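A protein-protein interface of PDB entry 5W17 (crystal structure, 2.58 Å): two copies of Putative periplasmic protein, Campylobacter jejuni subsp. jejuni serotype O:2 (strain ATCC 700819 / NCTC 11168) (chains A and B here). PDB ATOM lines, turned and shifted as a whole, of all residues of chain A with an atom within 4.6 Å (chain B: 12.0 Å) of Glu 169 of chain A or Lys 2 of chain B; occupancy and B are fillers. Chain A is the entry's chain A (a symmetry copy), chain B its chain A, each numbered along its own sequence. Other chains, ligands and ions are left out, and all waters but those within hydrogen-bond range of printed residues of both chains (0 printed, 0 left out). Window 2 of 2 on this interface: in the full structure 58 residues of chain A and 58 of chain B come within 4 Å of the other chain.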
ATOM      1  N   ILE A  36      20.405   7.953 -28.511  1.00  0.00           N
ATOM      2  CA  ILE A  36      21.849   7.879 -28.786  1.00  0.00           C
ATOM      3  C   ILE A  36      22.328   6.709 -29.690  1.00  0.00           C
ATOM      4  O   ILE A  36      22.278   5.537 -29.283  1.00  0.00           O
ATOM      5  CB  ILE A  36      22.631   7.827 -27.471  1.00  0.00           C
ATOM      6  CG1 ILE A  36      22.062   8.847 -26.484  1.00  0.00           C
ATOM      7  CG2 ILE A  36      24.118   8.031 -27.762  1.00  0.00           C
ATOM      8  CD1 ILE A  36      22.569   8.686 -25.067  1.00  0.00           C
ATOM      9  N   ASP A  37      22.806   7.047 -30.892  1.00  0.00           N
ATOM     10  CA  ASP A  37      23.446   6.108 -31.821  1.00  0.00           C
ATOM     11  C   ASP A  37      24.947   6.374 -31.905  1.00  0.00           C
ATOM     12  O   ASP A  37      25.389   7.470 -32.308  1.00  0.00           O
ATOM     13  CB  ASP A  37      22.876   6.230 -33.238  1.00  0.00           C
ATOM     14  CG  ASP A  37      21.453   5.668 -33.386  1.00  0.00           C
ATOM     15  OD1 ASP A  37      20.864   5.121 -32.405  1.00  0.00           O
ATOM     16  OD2 ASP A  37      20.930   5.786 -34.536  1.00  0.00           O
ATOM     17  N   PHE A  38      25.722   5.346 -31.571  1.00  0.00           N
ATOM     18  CA  PHE A  38      27.175   5.433 -31.513  1.00  0.00           C
ATOM     19  C   PHE A  38      27.840   4.143 -31.980  1.00  0.00           C
ATOM     20  O   PHE A  38      27.416   3.044 -31.621  1.00  0.00           O
ATOM     21  CB  PHE A  38      27.593   5.752 -30.074  1.00  0.00           C
ATOM     22  CG  PHE A  38      29.060   5.952 -29.887  1.00  0.00           C
ATOM     23  CD1 PHE A  38      29.703   7.063 -30.429  1.00  0.00           C
ATOM     24  CD2 PHE A  38      29.804   5.038 -29.142  1.00  0.00           C
ATOM     25  CE1 PHE A  38      31.067   7.247 -30.247  1.00  0.00           C
ATOM     26  CE2 PHE A  38      31.174   5.222 -28.955  1.00  0.00           C
ATOM     27  CZ  PHE A  38      31.802   6.329 -29.508  1.00  0.00           C
ATOM     28  N   PRO A  40      31.055   2.110 -31.589  1.00  0.00           N
ATOM     29  CA  PRO A  40      32.315   1.948 -30.848  1.00  0.00           C
ATOM     30  C   PRO A  40      33.500   1.443 -31.689  1.00  0.00           C
ATOM     31  O   PRO A  40      34.646   1.537 -31.253  1.00  0.00           O
ATOM     32  CB  PRO A  40      31.958   0.956 -29.731  1.00  0.00           C
ATOM     33  CG  PRO A  40      30.492   0.694 -29.864  1.00  0.00           C
ATOM     34  CD  PRO A  40      30.112   1.030 -31.267  1.00  0.00           C
ATOM     35  N   LYS A 128      27.351  -6.607 -22.787  1.00  0.00           N
ATOM     36  CA  LYS A 128      26.646  -5.519 -23.499  1.00  0.00           C
ATOM     37  C   LYS A 128      27.374  -4.167 -23.327  1.00  0.00           C
ATOM     38  O   LYS A 128      27.957  -3.882 -22.268  1.00  0.00           O
ATOM     39  CB  LYS A 128      25.194  -5.403 -23.026  1.00  0.00           C
ATOM     40  CG  LYS A 128      24.219  -6.390 -23.661  1.00  0.00           C
ATOM     41  CD  LYS A 128      23.056  -6.717 -22.721  1.00  0.00           C
ATOM     42  CE  LYS A 128      21.820  -5.845 -22.936  1.00  0.00           C
ATOM     43  NZ  LYS A 128      20.911  -6.410 -23.976  1.00  0.00           N
ATOM     44  N   GLU A 129      27.309  -3.341 -24.373  1.00  0.00           N
ATOM     45  CA  GLU A 129      28.061  -2.074 -24.480  1.00  0.00           C
ATOM     46  C   GLU A 129      27.775  -1.014 -23.406  1.00  0.00           C
ATOM     47  O   GLU A 129      26.684  -0.956 -22.808  1.00  0.00           O
ATOM     48  CB  GLU A 129      27.834  -1.435 -25.859  1.00  0.00           C
ATOM     49  CG  GLU A 129      28.369  -2.200 -27.063  1.00  0.00           C
ATOM     50  CD  GLU A 129      29.872  -2.091 -27.246  1.00  0.00           C
ATOM     51  OE1 GLU A 129      30.414  -2.998 -27.911  1.00  0.00           O
ATOM     52  OE2 GLU A 129      30.501  -1.114 -26.749  1.00  0.00           O
ATOM     53  N   ALA A 167      25.824   5.727 -20.524  1.00  0.00           N
ATOM     54  CA  ALA A 167      24.780   5.071 -21.319  1.00  0.00           C
ATOM     55  C   ALA A 167      25.113   3.617 -21.732  1.00  0.00           C
ATOM     56  O   ALA A 167      26.267   3.294 -22.068  1.00  0.00           O
ATOM     57  CB  ALA A 167      24.421   5.922 -22.530  1.00  0.00           C
ATOM     58  N   ASN A 168      24.081   2.768 -21.726  1.00  0.00           N
ATOM     59  CA  ASN A 168      24.201   1.332 -22.002  1.00  0.00           C
ATOM     60  C   ASN A 168      23.452   0.945 -23.245  1.00  0.00           C
ATOM     61  O   ASN A 168      22.524   1.623 -23.642  1.00  0.00           O
ATOM     62  CB  ASN A 168      23.662   0.549 -20.827  1.00  0.00           C
ATOM     63  CG  ASN A 168      24.280   0.996 -19.511  1.00  0.00           C
ATOM     64  OD1 ASN A 168      25.399   0.594 -19.151  1.00  0.00           O
ATOM     65  ND2 ASN A 168      23.560   1.847 -18.787  1.00  0.00           N
ATOM     66  N   GLU A 169      23.871  -0.149 -23.863  1.00  0.00           N
ATOM     67  CA  GLU A 169      23.231  -0.674 -25.073  1.00  0.00           C
ATOM     68  C   GLU A 169      21.735  -1.007 -24.850  1.00  0.00           C
ATOM     69  O   GLU A 169      21.331  -1.330 -23.730  1.00  0.00           O
ATOM     70  CB  GLU A 169      24.006  -1.905 -25.539  1.00  0.00           C
ATOM     71  CG  GLU A 169      23.951  -2.173 -27.037  1.00  0.00           C
ATOM     72  CD  GLU A 169      24.731  -3.416 -27.473  1.00  0.00           C
ATOM     73  OE1 GLU A 169      24.740  -3.706 -28.700  1.00  0.00           O
ATOM     74  OE2 GLU A 169      25.337  -4.103 -26.605  1.00  0.00           O
ATOM     75  N   LYS A 170      20.936  -0.933 -25.920  1.00  0.00           N
ATOM     76  CA  LYS A 170      19.466  -1.070 -25.870  1.00  0.00           C
ATOM     77  C   LYS A 170      18.969  -2.538 -25.958  1.00  0.00           C
ATOM     78  O   LYS A 170      19.780  -3.443 -26.177  1.00  0.00           O
ATOM     79  CB  LYS A 170      18.826  -0.200 -26.977  1.00  0.00           C
ATOM     80  CG  LYS A 170      17.767   0.777 -26.465  1.00  0.00           C
ATOM     81  CD  LYS A 170      16.764   1.217 -27.525  1.00  0.00           C
ATOM     82  CE  LYS A 170      15.475   1.745 -26.808  1.00  0.00           C
ATOM     83  NZ  LYS A 170      14.268   1.795 -27.714  1.00  0.00           N
ATOM     84  N   GLU A 171      17.646  -2.746 -25.789  1.00  0.00           N
ATOM     85  CA  GLU A 171      16.935  -4.064 -25.872  1.00  0.00           C
ATOM     86  C   GLU A 171      17.502  -5.122 -24.926  1.00  0.00           C
ATOM     87  O   GLU A 171      18.027  -4.790 -23.856  1.00  0.00           O
ATOM     88  CB  GLU A 171      16.838  -4.605 -27.319  1.00  0.00           C
ATOM     89  N   MET B   1      27.202   0.536 -36.284  1.00  0.00           N
ATOM     90  CA  MET B   1      26.715   1.380 -35.148  1.00  0.00           C
ATOM     91  C   MET B   1      25.863   0.602 -34.126  1.00  0.00           C
ATOM     92  O   MET B   1      25.674  -0.586 -34.276  1.00  0.00           O
ATOM     93  CB  MET B   1      26.040   2.657 -35.679  1.00  0.00           C
ATOM     94  CG  MET B   1      24.702   2.458 -36.361  1.00  0.00           C
ATOM     95  SD  MET B   1      23.410   3.037 -35.240  1.00  0.00           S
ATOM     96  CE  MET B   1      22.490   1.544 -34.806  1.00  0.00           C
ATOM     97  N   LYS B   2      25.375   1.282 -33.093  1.00  0.00           N
ATOM     98  CA  LYS B   2      24.763   0.661 -31.917  1.00  0.00           C
ATOM     99  C   LYS B   2      23.979   1.729 -31.159  1.00  0.00           C
ATOM    100  O   LYS B   2      24.376   2.892 -31.140  1.00  0.00           O
ATOM    101  CB  LYS B   2      25.846   0.079 -31.003  1.00  0.00           C
ATOM    102  CG  LYS B   2      25.917  -1.432 -30.955  1.00  0.00           C
ATOM    103  CD  LYS B   2      27.366  -1.918 -30.986  1.00  0.00           C
ATOM    104  CE  LYS B   2      27.568  -3.315 -30.384  1.00  0.00           C
ATOM    105  NZ  LYS B   2      26.742  -4.407 -30.986  1.00  0.00           N
ATOM    106  N   GLU B   3      22.888   1.331 -30.512  1.00  0.00           N
ATOM    107  CA  GLU B   3      21.974   2.259 -29.829  1.00  0.00           C
ATOM    108  C   GLU B   3      22.102   2.134 -28.331  1.00  0.00           C
ATOM    109  O   GLU B   3      22.280   1.034 -27.810  1.00  0.00           O
ATOM    110  CB  GLU B   3      20.527   1.979 -30.208  1.00  0.00           C
ATOM    111  CG  GLU B   3      20.272   1.921 -31.703  1.00  0.00           C
ATOM    112  CD  GLU B   3      18.816   1.674 -32.040  1.00  0.00           C
ATOM    113  OE1 GLU B   3      18.565   0.982 -33.051  1.00  0.00           O
ATOM    114  OE2 GLU B   3      17.931   2.172 -31.297  1.00  0.00           O
ATOM    115  N   TYR B   4      22.007   3.264 -27.632  1.00  0.00           N
ATOM    116  CA  TYR B   4      22.185   3.263 -26.179  1.00  0.00           C
ATOM    117  C   TYR B   4      21.014   3.937 -25.480  1.00  0.00           C
ATOM    118  O   TYR B   4      20.211   4.599 -26.121  1.00  0.00           O
ATOM    119  CB  TYR B   4      23.495   3.941 -25.792  1.00  0.00           C
ATOM    120  CG  TYR B   4      24.742   3.356 -26.409  1.00  0.00           C
ATOM    121  CD1 TYR B   4      24.997   3.437 -27.814  1.00  0.00           C
ATOM    122  CD2 TYR B   4      25.716   2.764 -25.589  1.00  0.00           C
ATOM    123  CE1 TYR B   4      26.162   2.906 -28.370  1.00  0.00           C
ATOM    124  CE2 TYR B   4      26.900   2.252 -26.136  1.00  0.00           C
ATOM    125  CZ  TYR B   4      27.115   2.319 -27.515  1.00  0.00           C
ATOM    126  OH  TYR B   4      28.287   1.800 -28.005  1.00  0.00           O
ATOM    127  N   THR B   5      20.911   3.744 -24.175  1.00  0.00           N
ATOM    128  CA  THR B   5      19.875   4.375 -23.387  1.00  0.00           C
ATOM    129  C   THR B   5      20.635   4.959 -22.244  1.00  0.00           C
ATOM    130  O   THR B   5      21.460   4.269 -21.617  1.00  0.00           O
ATOM    131  CB  THR B   5      18.798   3.368 -22.876  1.00  0.00           C
ATOM    132  OG1 THR B   5      18.081   2.819 -23.992  1.00  0.00           O
ATOM    133  CG2 THR B   5      17.773   4.045 -21.914  1.00  0.00           C
ATOM    134  N   LEU B   6      20.360   6.228 -21.973  1.00  0.00           N
ATOM    135  CA  LEU B   6      21.031   6.938 -20.890  1.00  0.00           C
ATOM    136  C   LEU B   6      20.833   6.203 -19.580  1.00  0.00           C
ATOM    137  O   LEU B   6      19.831   5.525 -19.393  1.00  0.00           O
ATOM    138  CB  LEU B   6      20.473   8.345 -20.739  1.00  0.00           C
ATOM    139  CG  LEU B   6      20.328   9.193 -21.977  1.00  0.00           C
ATOM    140  CD1 LEU B   6      18.898   9.098 -22.487  1.00  0.00           C
ATOM    141  CD2 LEU B   6      20.668  10.590 -21.534  1.00  0.00           C
ATOM    142  N   ASP B   7      21.807   6.309 -18.694  1.00  0.00           N
ATOM    143  CA  ASP B   7      21.631   5.895 -17.319  1.00  0.00           C
ATOM    144  C   ASP B   7      21.358   7.218 -16.621  1.00  0.00           C
ATOM    145  O   ASP B   7      22.286   7.964 -16.300  1.00  0.00           O
ATOM    146  CB  ASP B   7      22.898   5.155 -16.812  1.00  0.00           C
ATOM    147  CG  ASP B   7      22.940   4.945 -15.280  1.00  0.00           C
ATOM    148  OD1 ASP B   7      21.962   5.281 -14.554  1.00  0.00           O
ATOM    149  OD2 ASP B   7      23.987   4.428 -14.802  1.00  0.00           O
ATOM    150  N   LYS B   8      20.074   7.520 -16.429  1.00  0.00           N
ATOM    151  CA  LYS B   8      19.632   8.762 -15.789  1.00  0.00           C
ATOM    152  C   LYS B   8      20.329   9.032 -14.433  1.00  0.00           C
ATOM    153  O   LYS B   8      20.571  10.194 -14.070  1.00  0.00           O
ATOM    154  CB  LYS B   8      18.111   8.775 -15.632  1.00  0.00           C
ATOM    155  CG  LYS B   8      17.322   9.255 -16.841  1.00  0.00           C
ATOM    156  CD  LYS B   8      16.086  10.023 -16.343  1.00  0.00           C
ATOM    157  CE  LYS B   8      14.859   9.922 -17.250  1.00  0.00           C
ATOM    158  NZ  LYS B   8      15.169  10.050 -18.704  1.00  0.00           N
ATOM    159  N   THR B  11      23.969  10.555 -15.283  1.00  0.00           N
ATOM    160  CA  THR B  11      23.894  11.550 -16.349  1.00  0.00           C
ATOM    161  C   THR B  11      23.419  12.863 -15.733  1.00  0.00           C
ATOM    162  O   THR B  11      22.450  12.889 -14.971  1.00  0.00           O
ATOM    163  CB  THR B  11      22.971  11.080 -17.509  1.00  0.00           C
ATOM    164  OG1 THR B  11      23.589   9.992 -18.219  1.00  0.00           O
ATOM    165  CG2 THR B  11      22.685  12.195 -18.495  1.00  0.00           C
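Among the printed residues, merely in contact across the chains: Asn 168 of chain A with Tyr 4 of chain B (3.0 Å), Pro 40 of chain A with Tyr 4 of chain B (3.1 Å), Lys 170 of chain A with Thr 5 of chain B (3.2 Å), Asp 37 of chain A with Glu 3 of chain B (3.3 Å), Ile 36 of chain A with Glu 3 of chain B (3.3 Å), Glu 169 of chain A with Glu 3 of chain B (3.4 Å), Asp 37 of chain A with Lys 2 of chain B (3.4 Å), Ala 167 of chain A with Thr 5 of chain B (3.4 Å), Phe 38 of chain A with Tyr 4 of chain B (3.5 Å), Glu 129 of chain A with Lys 2 of chain B (3.6 Å), Ala 167 of chain A with Tyr 4 of chain B (3.6 Å), Glu 129 of chain A with Tyr 4 of chain B (3.8 Å), Phe 38 of chain A with Met 1 of chain B (3.8 Å), Ile 36 of chain A with Leu 6 of chain B (3.9 Å), Ile 36 of chain A with Lys 2 of chain B (3.9 Å), Glu 169 of chain A with Tyr 4 of chain B (3.9 Å), Ala 167 of chain A with Leu 6 of chain B (3.9 Å) and Asn 168 of chain A with Asp 7 of chain B (3.9 Å).
N of Phe 38 of chain A sits at hydrogen-bond distance from O of Lys 2 of chain B (2.8 Å).
The backbone NH of Tyr 4 of chain B lies within hydrogen-bond range of the backbone carbonyl oxygen of Ile 36 of chain A (2.8 Å).
The backbone carbonyl oxygen (O) of Glu 3 of chain B sits at hydrogen-bond distance from the backbone NH (N) of Lys 170 of chain A (3.0 Å).
SD of Met 1 of chain B lies close to OD2 of Asp 37 of chain A, 3.8 Å away.
The side-chain amino group (NZ) of Lys 2 of chain B is in salt-bridge range of the side-chain carboxylate (OE1) of Glu 169 of chain A, at 3.1 Å.
The backbone NH of Thr 5 of chain B lies within hydrogen-bond range of the backbone carbonyl oxygen of Asn 168 of chain A (2.7 Å).
No position is printed for both chains.
Glu 169 of chain A touches just these residues of chain B: Lys 2, Glu 3 and Tyr 4.
Of the printed residues of chain A, Lys 2 of chain B touches Ile 36 (3.9 Å), Asp 37 (3.4 Å), Phe 38 (2.8 Å), Glu 129 (3.6 Å) and Glu 169 (3.1 Å).
Asp 37 of chain A touches just these residues of chain B: Met 1, Lys 2 and Glu 3.
No residue of chain B comes within 4 Å of Lys 128 of chain A.
Of the printed residues of chain B, Glu 129 of chain A touches Lys 2 and Tyr 4.
Of chain B, only Tyr 4 (3.0 Å), Thr 5 (2.7 Å) and Asp 7 (3.9 Å) come within 4 Å of Asn 168 of chain A.
No residue of chain B comes within 4 Å of Glu 171 of chain A.
Printed residues of chain B within 4 Å of Pro 40 of chain A: Tyr 4 (3.1 Å).
Of the printed residues of chain A, Thr 5 of chain B touches Ala 167, Asn 168 and Lys 170.
Of the printed residues of chain A, Met 1 of chain B touches Asp 37 (3.8 Å) and Phe 38 (3.8 Å).
Printed residues of chain A within 4 Å of Leu 6 of chain B: Ile 36 (3.9 Å) and Ala 167 (3.9 Å).
The nearest residue of chain A that does not touch Lys 2 of chain B is Pro 40 of chain A (4.04 Å).
The side-chain hydroxyl (OG1) of Thr 11 of chain B sits at hydrogen-bond distance from the backbone carbonyl oxygen (O) of Asp 7 of chain B, 3.1 Å away.
The backbone NH of Glu 129 of chain A is in hydrogen-bond range of the side-chain carboxylate of Glu 169 of chain A (3.1 Å).
Of the 11 printed residues of chain A, 9 touch a printed residue of chain B.
Hydrophobic or aromatic side chains of chain A that line the printed part of chain B: Ile 36, Phe 38, Pro 40 and Ala 167.
Hydrophobic or aromatic side chains of chain B within 4 Å of the printed part of chain A: Met 1, Tyr 4 and Leu 6.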
